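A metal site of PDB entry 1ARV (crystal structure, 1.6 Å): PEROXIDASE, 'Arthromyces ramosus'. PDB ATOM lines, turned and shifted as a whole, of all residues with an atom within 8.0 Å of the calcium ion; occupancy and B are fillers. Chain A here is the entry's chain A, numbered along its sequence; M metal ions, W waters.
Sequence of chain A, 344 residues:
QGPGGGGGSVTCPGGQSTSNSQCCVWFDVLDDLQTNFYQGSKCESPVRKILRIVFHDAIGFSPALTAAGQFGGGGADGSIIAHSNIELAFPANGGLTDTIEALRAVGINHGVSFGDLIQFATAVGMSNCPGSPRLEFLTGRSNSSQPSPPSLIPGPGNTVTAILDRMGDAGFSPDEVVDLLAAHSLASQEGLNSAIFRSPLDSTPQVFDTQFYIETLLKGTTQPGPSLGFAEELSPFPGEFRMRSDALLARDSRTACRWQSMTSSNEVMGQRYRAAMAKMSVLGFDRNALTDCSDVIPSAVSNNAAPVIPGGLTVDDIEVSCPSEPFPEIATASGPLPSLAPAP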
ATOM      1  N   ILE A  53     -23.744  29.974 -16.625  1.00  0.00           N
ATOM      2  CA  ILE A  53     -23.306  29.320 -15.406  1.00  0.00           C
ATOM      3  C   ILE A  53     -23.930  29.966 -14.159  1.00  0.00           C
ATOM      4  O   ILE A  53     -24.403  29.221 -13.291  1.00  0.00           O
ATOM      5  CB  ILE A  53     -21.750  29.373 -15.345  1.00  0.00           C
ATOM      6  CG1 ILE A  53     -21.181  28.392 -16.379  1.00  0.00           C
ATOM      7  CG2 ILE A  53     -21.243  29.009 -13.946  1.00  0.00           C
ATOM      8  CD1 ILE A  53     -19.682  28.641 -16.657  1.00  0.00           C
ATOM      9  N   VAL A  54     -24.020  31.282 -14.016  1.00  0.00           N
ATOM     10  CA  VAL A  54     -24.558  31.831 -12.784  1.00  0.00           C
ATOM     11  C   VAL A  54     -26.025  31.440 -12.611  1.00  0.00           C
ATOM     12  O   VAL A  54     -26.438  31.079 -11.512  1.00  0.00           O
ATOM     13  CB  VAL A  54     -24.281  33.364 -12.793  1.00  0.00           C
ATOM     14  CG1 VAL A  54     -25.141  34.128 -13.798  1.00  0.00           C
ATOM     15  CG2 VAL A  54     -24.492  33.884 -11.380  1.00  0.00           C
ATOM     16  N   PHE A  55     -26.787  31.411 -13.731  1.00  0.00           N
ATOM     17  CA  PHE A  55     -28.181  31.020 -13.739  1.00  0.00           C
ATOM     18  C   PHE A  55     -28.273  29.543 -13.396  1.00  0.00           C
ATOM     19  O   PHE A  55     -28.979  29.173 -12.450  1.00  0.00           O
ATOM     20  CB  PHE A  55     -28.781  31.270 -15.145  1.00  0.00           C
ATOM     21  CG  PHE A  55     -30.233  30.798 -15.390  1.00  0.00           C
ATOM     22  CD1 PHE A  55     -31.204  30.861 -14.400  1.00  0.00           C
ATOM     23  CD2 PHE A  55     -30.586  30.296 -16.619  1.00  0.00           C
ATOM     24  CE1 PHE A  55     -32.491  30.431 -14.646  1.00  0.00           C
ATOM     25  CE2 PHE A  55     -31.873  29.866 -16.866  1.00  0.00           C
ATOM     26  CZ  PHE A  55     -32.819  29.931 -15.878  1.00  0.00           C
ATOM     27  N   HIS A  56     -27.493  28.666 -14.047  1.00  0.00           N
ATOM     28  CA  HIS A  56     -27.585  27.232 -13.811  1.00  0.00           C
ATOM     29  C   HIS A  56     -27.139  26.799 -12.447  1.00  0.00           C
ATOM     30  O   HIS A  56     -27.597  25.789 -11.900  1.00  0.00           O
ATOM     31  CB  HIS A  56     -26.811  26.488 -14.878  1.00  0.00           C
ATOM     32  CG  HIS A  56     -27.441  26.597 -16.264  1.00  0.00           C
ATOM     33  ND1 HIS A  56     -27.139  25.863 -17.317  1.00  0.00           N
ATOM     34  CD2 HIS A  56     -28.386  27.497 -16.692  1.00  0.00           C
ATOM     35  CE1 HIS A  56     -27.836  26.275 -18.349  1.00  0.00           C
ATOM     36  NE2 HIS A  56     -28.582  27.262 -17.963  1.00  0.00           N
ATOM     37  N   ASP A  57     -26.242  27.573 -11.852  1.00  0.00           N
ATOM     38  CA  ASP A  57     -25.815  27.310 -10.503  1.00  0.00           C
ATOM     39  C   ASP A  57     -26.905  27.756  -9.528  1.00  0.00           C
ATOM     40  O   ASP A  57     -27.319  26.928  -8.700  1.00  0.00           O
ATOM     41  CB  ASP A  57     -24.514  28.069 -10.152  1.00  0.00           C
ATOM     42  CG  ASP A  57     -24.007  27.780  -8.751  1.00  0.00           C
ATOM     43  OD1 ASP A  57     -24.190  26.649  -8.281  1.00  0.00           O
ATOM     44  OD2 ASP A  57     -23.419  28.687  -8.165  1.00  0.00           O
ATOM     45  N   ALA A  58     -27.396  28.985  -9.633  1.00  0.00           N
ATOM     46  CA  ALA A  58     -28.363  29.518  -8.704  1.00  0.00           C
ATOM     47  C   ALA A  58     -29.728  28.890  -8.726  1.00  0.00           C
ATOM     48  O   ALA A  58     -30.335  28.676  -7.677  1.00  0.00           O
ATOM     49  CB  ALA A  58     -28.527  31.021  -8.953  1.00  0.00           C
ATOM     50  N   ILE A  59     -30.242  28.545  -9.912  1.00  0.00           N
ATOM     51  CA  ILE A  59     -31.558  27.973 -10.031  1.00  0.00           C
ATOM     52  C   ILE A  59     -31.667  26.546  -9.488  1.00  0.00           C
ATOM     53  O   ILE A  59     -32.793  26.053  -9.415  1.00  0.00           O
ATOM     54  CB  ILE A  59     -32.007  28.088 -11.539  1.00  0.00           C
ATOM     55  CG1 ILE A  59     -33.521  28.235 -11.594  1.00  0.00           C
ATOM     56  CG2 ILE A  59     -31.525  26.894 -12.373  1.00  0.00           C
ATOM     57  CD1 ILE A  59     -34.039  29.516 -10.953  1.00  0.00           C
ATOM     58  N   GLY A  60     -30.574  25.851  -9.105  1.00  0.00           N
ATOM     59  CA  GLY A  60     -30.702  24.535  -8.513  1.00  0.00           C
ATOM     60  C   GLY A  60     -31.080  24.782  -7.053  1.00  0.00           C
ATOM     61  O   GLY A  60     -30.279  24.619  -6.110  1.00  0.00           O
ATOM     62  N   PHE A  61     -32.327  25.211  -6.882  1.00  0.00           N
ATOM     63  CA  PHE A  61     -32.883  25.546  -5.600  1.00  0.00           C
ATOM     64  C   PHE A  61     -34.386  25.304  -5.698  1.00  0.00           C
ATOM     65  O   PHE A  61     -35.074  25.946  -6.485  1.00  0.00           O
ATOM     66  CB  PHE A  61     -32.564  27.011  -5.328  1.00  0.00           C
ATOM     67  CG  PHE A  61     -33.076  27.472  -3.970  1.00  0.00           C
ATOM     68  CD1 PHE A  61     -32.473  27.011  -2.836  1.00  0.00           C
ATOM     69  CD2 PHE A  61     -34.146  28.351  -3.911  1.00  0.00           C
ATOM     70  CE1 PHE A  61     -32.958  27.433  -1.617  1.00  0.00           C
ATOM     71  CE2 PHE A  61     -34.618  28.755  -2.683  1.00  0.00           C
ATOM     72  CZ  PHE A  61     -34.022  28.306  -1.529  1.00  0.00           C
ATOM     73  N   GLY A  73     -31.469  21.433  -3.214  1.00  0.00           N
ATOM     74  CA  GLY A  73     -30.410  22.195  -3.864  1.00  0.00           C
ATOM     75  C   GLY A  73     -29.990  23.354  -2.988  1.00  0.00           C
ATOM     76  O   GLY A  73     -30.798  23.862  -2.214  1.00  0.00           O
ATOM     77  N   GLY A  74     -28.730  23.771  -3.035  1.00  0.00           N
ATOM     78  CA  GLY A  74     -28.256  24.858  -2.193  1.00  0.00           C
ATOM     79  C   GLY A  74     -28.251  26.211  -2.881  1.00  0.00           C
ATOM     80  O   GLY A  74     -27.672  27.157  -2.324  1.00  0.00           O
ATOM     81  N   GLY A  75     -28.837  26.369  -4.069  1.00  0.00           N
ATOM     82  CA  GLY A  75     -28.856  27.662  -4.713  1.00  0.00           C
ATOM     83  C   GLY A  75     -27.500  28.102  -5.253  1.00  0.00           C
ATOM     84  O   GLY A  75     -26.801  27.299  -5.890  1.00  0.00           O
ATOM     85  N   ALA A  76     -27.110  29.345  -4.980  1.00  0.00           N
ATOM     86  CA  ALA A  76     -25.909  29.946  -5.540  1.00  0.00           C
ATOM     87  C   ALA A  76     -24.685  29.577  -4.733  1.00  0.00           C
ATOM     88  O   ALA A  76     -23.905  30.412  -4.290  1.00  0.00           O
ATOM     89  CB  ALA A  76     -26.119  31.456  -5.574  1.00  0.00           C
ATOM     90  N   ASP A  77     -24.476  28.268  -4.664  1.00  0.00           N
ATOM     91  CA  ASP A  77     -23.434  27.647  -3.857  1.00  0.00           C
ATOM     92  C   ASP A  77     -22.183  27.165  -4.577  1.00  0.00           C
ATOM     93  O   ASP A  77     -21.315  26.514  -3.978  1.00  0.00           O
ATOM     94  CB  ASP A  77     -24.101  26.481  -3.088  1.00  0.00           C
ATOM     95  CG  ASP A  77     -24.704  25.407  -3.992  1.00  0.00           C
ATOM     96  OD1 ASP A  77     -24.612  25.518  -5.212  1.00  0.00           O
ATOM     97  OD2 ASP A  77     -25.271  24.443  -3.472  1.00  0.00           O
ATOM     98  N   GLY A  78     -22.071  27.417  -5.883  1.00  0.00           N
ATOM     99  CA  GLY A  78     -20.902  26.948  -6.633  1.00  0.00           C
ATOM    100  C   GLY A  78     -20.894  25.447  -6.862  1.00  0.00           C
ATOM    101  O   GLY A  78     -19.888  24.917  -7.337  1.00  0.00           O
ATOM    102  N   SER A  79     -22.043  24.766  -6.669  1.00  0.00           N
ATOM    103  CA  SER A  79     -22.071  23.314  -6.810  1.00  0.00           C
ATOM    104  C   SER A  79     -21.835  22.937  -8.251  1.00  0.00           C
ATOM    105  O   SER A  79     -21.326  21.840  -8.442  1.00  0.00           O
ATOM    106  CB  SER A  79     -23.404  22.725  -6.385  1.00  0.00           C
ATOM    107  OG  SER A  79     -24.486  23.274  -7.180  1.00  0.00           O
ATOM    108  N   ILE A  80     -22.161  23.772  -9.256  1.00  0.00           N
ATOM    109  CA  ILE A  80     -21.868  23.423 -10.648  1.00  0.00           C
ATOM    110  C   ILE A  80     -20.352  23.270 -10.867  1.00  0.00           C
ATOM    111  O   ILE A  80     -19.949  22.605 -11.812  1.00  0.00           O
ATOM    112  CB  ILE A  80     -22.524  24.531 -11.576  1.00  0.00           C
ATOM    113  CG1 ILE A  80     -22.535  24.049 -13.047  1.00  0.00           C
ATOM    114  CG2 ILE A  80     -21.774  25.863 -11.444  1.00  0.00           C
ATOM    115  CD1 ILE A  80     -23.451  24.899 -13.939  1.00  0.00           C
ATOM    116  N   ILE A  81     -19.471  23.844 -10.049  1.00  0.00           N
ATOM    117  CA  ILE A  81     -18.038  23.641 -10.185  1.00  0.00           C
ATOM    118  C   ILE A  81     -17.610  22.492  -9.253  1.00  0.00           C
ATOM    119  O   ILE A  81     -17.042  21.486  -9.719  1.00  0.00           O
ATOM    120  CB  ILE A  81     -17.221  24.911  -9.810  1.00  0.00           C
ATOM    121  CG1 ILE A  81     -17.625  26.088 -10.686  1.00  0.00           C
ATOM    122  CG2 ILE A  81     -15.738  24.618  -9.996  1.00  0.00           C
ATOM    123  CD1 ILE A  81     -16.802  27.376 -10.504  1.00  0.00           C
ATOM    124  N   HIS A  83     -19.181  20.073  -7.952  1.00  0.00           N
ATOM    125  CA  HIS A  83     -19.812  18.832  -8.383  1.00  0.00           C
ATOM    126  C   HIS A  83     -20.072  18.829  -9.878  1.00  0.00           C
ATOM    127  O   HIS A  83     -21.098  18.296 -10.334  1.00  0.00           O
ATOM    128  CB  HIS A  83     -21.127  18.625  -7.641  1.00  0.00           C
ATOM    129  CG  HIS A  83     -20.808  18.541  -6.151  1.00  0.00           C
ATOM    130  ND1 HIS A  83     -20.124  17.496  -5.527  1.00  0.00           N
ATOM    131  CD2 HIS A  83     -21.172  19.539  -5.226  1.00  0.00           C
ATOM    132  CE1 HIS A  83     -20.092  17.857  -4.220  1.00  0.00           C
ATOM    133  NE2 HIS A  83     -20.673  19.004  -4.028  1.00  0.00           N
ATOM    134  N   GLU A  87     -23.198  17.573 -12.288  1.00  0.00           N
ATOM    135  CA  GLU A  87     -24.060  18.568 -12.906  1.00  0.00           C
ATOM    136  C   GLU A  87     -23.855  18.855 -14.380  1.00  0.00           C
ATOM    137  O   GLU A  87     -24.798  19.191 -15.102  1.00  0.00           O
ATOM    138  CB  GLU A  87     -23.965  19.888 -12.141  1.00  0.00           C
ATOM    139  CG  GLU A  87     -24.558  19.773 -10.748  1.00  0.00           C
ATOM    140  CD  GLU A  87     -24.760  21.121 -10.071  1.00  0.00           C
ATOM    141  OE1 GLU A  87     -25.016  22.102 -10.763  1.00  0.00           O
ATOM    142  OE2 GLU A  87     -24.659  21.161  -8.845  1.00  0.00           O
ATOM    143  N   GLY A 115     -19.024  29.566  -5.040  1.00  0.00           N
ATOM    144  CA  GLY A 115     -20.292  30.313  -5.162  1.00  0.00           C
ATOM    145  C   GLY A 115     -20.040  31.788  -5.249  1.00  0.00           C
ATOM    146  O   GLY A 115     -20.618  32.459  -6.106  1.00  0.00           O
ATOM    147  N   ILE A 118     -18.362  32.704  -8.815  1.00  0.00           N
ATOM    148  CA  ILE A 118     -19.277  32.769  -9.942  1.00  0.00           C
ATOM    149  C   ILE A 118     -20.022  34.096  -9.930  1.00  0.00           C
ATOM    150  O   ILE A 118     -20.110  34.734 -10.978  1.00  0.00           O
ATOM    151  CB  ILE A 118     -20.214  31.552  -9.856  1.00  0.00           C
ATOM    152  CG1 ILE A 118     -19.448  30.288 -10.252  1.00  0.00           C
ATOM    153  CG2 ILE A 118     -21.391  31.744 -10.802  1.00  0.00           C
ATOM    154  CD1 ILE A 118     -20.244  28.987  -9.988  1.00  0.00           C
ATOM    155  N   SER A 145     -20.900  22.464  -0.695  1.00  0.00           N
ATOM    156  CA  SER A 145     -22.133  22.288  -1.415  1.00  0.00           C
ATOM    157  C   SER A 145     -22.398  20.798  -1.655  1.00  0.00           C
ATOM    158  O   SER A 145     -21.518  19.934  -1.542  1.00  0.00           O
ATOM    159  CB  SER A 145     -22.035  23.022  -2.741  1.00  0.00           C
ATOM    160  OG  SER A 145     -20.918  22.517  -3.460  1.00  0.00           O
ATOM    161  N   GLN A 146     -23.666  20.478  -1.888  1.00  0.00           N
ATOM    162  CA  GLN A 146     -24.086  19.150  -2.271  1.00  0.00           C
ATOM    163  C   GLN A 146     -24.477  19.313  -3.738  1.00  0.00           C
ATOM    164  O   GLN A 146     -24.783  20.439  -4.177  1.00  0.00           O
ATOM    165  CB  GLN A 146     -25.311  18.712  -1.517  1.00  0.00           C
ATOM    166  CG  GLN A 146     -25.122  18.160  -0.122  1.00  0.00           C
ATOM    167  CD  GLN A 146     -26.487  17.764   0.439  1.00  0.00           C
ATOM    168  OE1 GLN A 146     -27.175  16.877  -0.067  1.00  0.00           O
ATOM    169  NE2 GLN A 146     -26.974  18.420   1.482  1.00  0.00           N
ATOM    170  N   PRO A 147     -24.501  18.265  -4.576  1.00  0.00           N
ATOM    171  CA  PRO A 147     -24.895  18.336  -5.973  1.00  0.00           C
ATOM    172  C   PRO A 147     -26.316  18.834  -6.124  1.00  0.00           C
ATOM    173  O   PRO A 147     -27.172  18.514  -5.300  1.00  0.00           O
ATOM    174  CB  PRO A 147     -24.750  16.932  -6.511  1.00  0.00           C
ATOM    175  CG  PRO A 147     -23.720  16.335  -5.590  1.00  0.00           C
ATOM    176  CD  PRO A 147     -24.136  16.890  -4.247  1.00  0.00           C
ATOM    177  N   SER A 148     -26.566  19.623  -7.179  1.00  0.00           N
ATOM    178  CA  SER A 148     -27.920  20.083  -7.433  1.00  0.00           C
ATOM    179  C   SER A 148     -28.753  18.864  -7.817  1.00  0.00           C
ATOM    180  O   SER A 148     -28.240  17.954  -8.485  1.00  0.00           O
ATOM    181  CB  SER A 148     -27.954  21.080  -8.599  1.00  0.00           C
ATOM    182  OG  SER A 148     -29.292  21.458  -8.952  1.00  0.00           O
ATOM    183  N   PRO A 149     -30.043  18.801  -7.420  1.00  0.00           N
ATOM    184  CA  PRO A 149     -30.971  17.803  -7.926  1.00  0.00           C
ATOM    185  C   PRO A 149     -31.074  18.020  -9.442  1.00  0.00           C
ATOM    186  O   PRO A 149     -30.830  19.140  -9.929  1.00  0.00           O
ATOM    187  CB  PRO A 149     -32.272  18.064  -7.178  1.00  0.00           C
ATOM    188  CG  PRO A 149     -31.794  18.694  -5.884  1.00  0.00           C
ATOM    189  CD  PRO A 149     -30.631  19.577  -6.322  1.00  0.00           C
ATOM    190  N   LEU A 283     -29.984  33.056  -3.635  1.00  0.00           N
ATOM    191  CA  LEU A 283     -30.882  31.913  -3.475  1.00  0.00           C
ATOM    192  C   LEU A 283     -30.094  30.854  -2.686  1.00  0.00           C
ATOM    193  O   LEU A 283     -28.963  30.508  -3.015  1.00  0.00           O
ATOM    194  CB  LEU A 283     -31.276  31.393  -4.894  1.00  0.00           C
ATOM    195  CG  LEU A 283     -32.675  31.557  -5.553  1.00  0.00           C
ATOM    196  CD1 LEU A 283     -33.342  32.891  -5.280  1.00  0.00           C
ATOM    197  CD2 LEU A 283     -32.470  31.293  -7.033  1.00  0.00           C
ATOM    198  N   PHE A 285     -29.199  31.437   0.516  1.00  0.00           N
ATOM    199  CA  PHE A 285     -28.418  32.172   1.513  1.00  0.00           C
ATOM    200  C   PHE A 285     -29.228  33.288   2.141  1.00  0.00           C
ATOM    201  O   PHE A 285     -30.292  33.681   1.649  1.00  0.00           O
ATOM    202  CB  PHE A 285     -27.171  32.827   0.869  1.00  0.00           C
ATOM    203  CG  PHE A 285     -26.197  31.758   0.412  1.00  0.00           C
ATOM    204  CD1 PHE A 285     -26.358  31.183  -0.839  1.00  0.00           C
ATOM    205  CD2 PHE A 285     -25.243  31.272   1.284  1.00  0.00           C
ATOM    206  CE1 PHE A 285     -25.564  30.111  -1.210  1.00  0.00           C
ATOM    207  CE2 PHE A 285     -24.454  30.203   0.905  1.00  0.00           C
ATOM    208  CZ  PHE A 285     -24.618  29.628  -0.332  1.00  0.00           C
HETATM  209 CA    CA M   1     -25.893  25.361  -7.305  1.00  0.00          CA
HETATM  210  O   HOH W   1     -26.356  24.224  -9.495  1.00  0.00           O
HETATM  211  O   HOH W   2     -27.663  23.964  -6.582  1.00  0.00           O
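The backbone NH (N) of Gly 78 is in hydrogen-bond range of the side-chain carboxylate (OD2) of Asp 57.
The side-chain hydroxyl of Ser 79 lies close to the side-chain carboxylate of Glu 87 (2.7 Å).
The backbone NH of Gly 75 sits at hydrogen-bond distance from the backbone carbonyl oxygen of Gly 60 (3.1 Å).
Of the 29 residues printed, 4 come within 4 Å of the calcium ion.
The calcium ion is bound by OD1 of Asp 57, water W2, OD1 of Asp 77, water W1, OG of Ser 79, O of Asp 57 and O of Gly 75.
The calcium ion has seven donor atoms within binding distance.
Water W1 bridges the side-chain carboxylate (OE1) of Glu 87 (2.8 Å) and the backbone carbonyl oxygen (O) of His 56 (3.1 Å).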
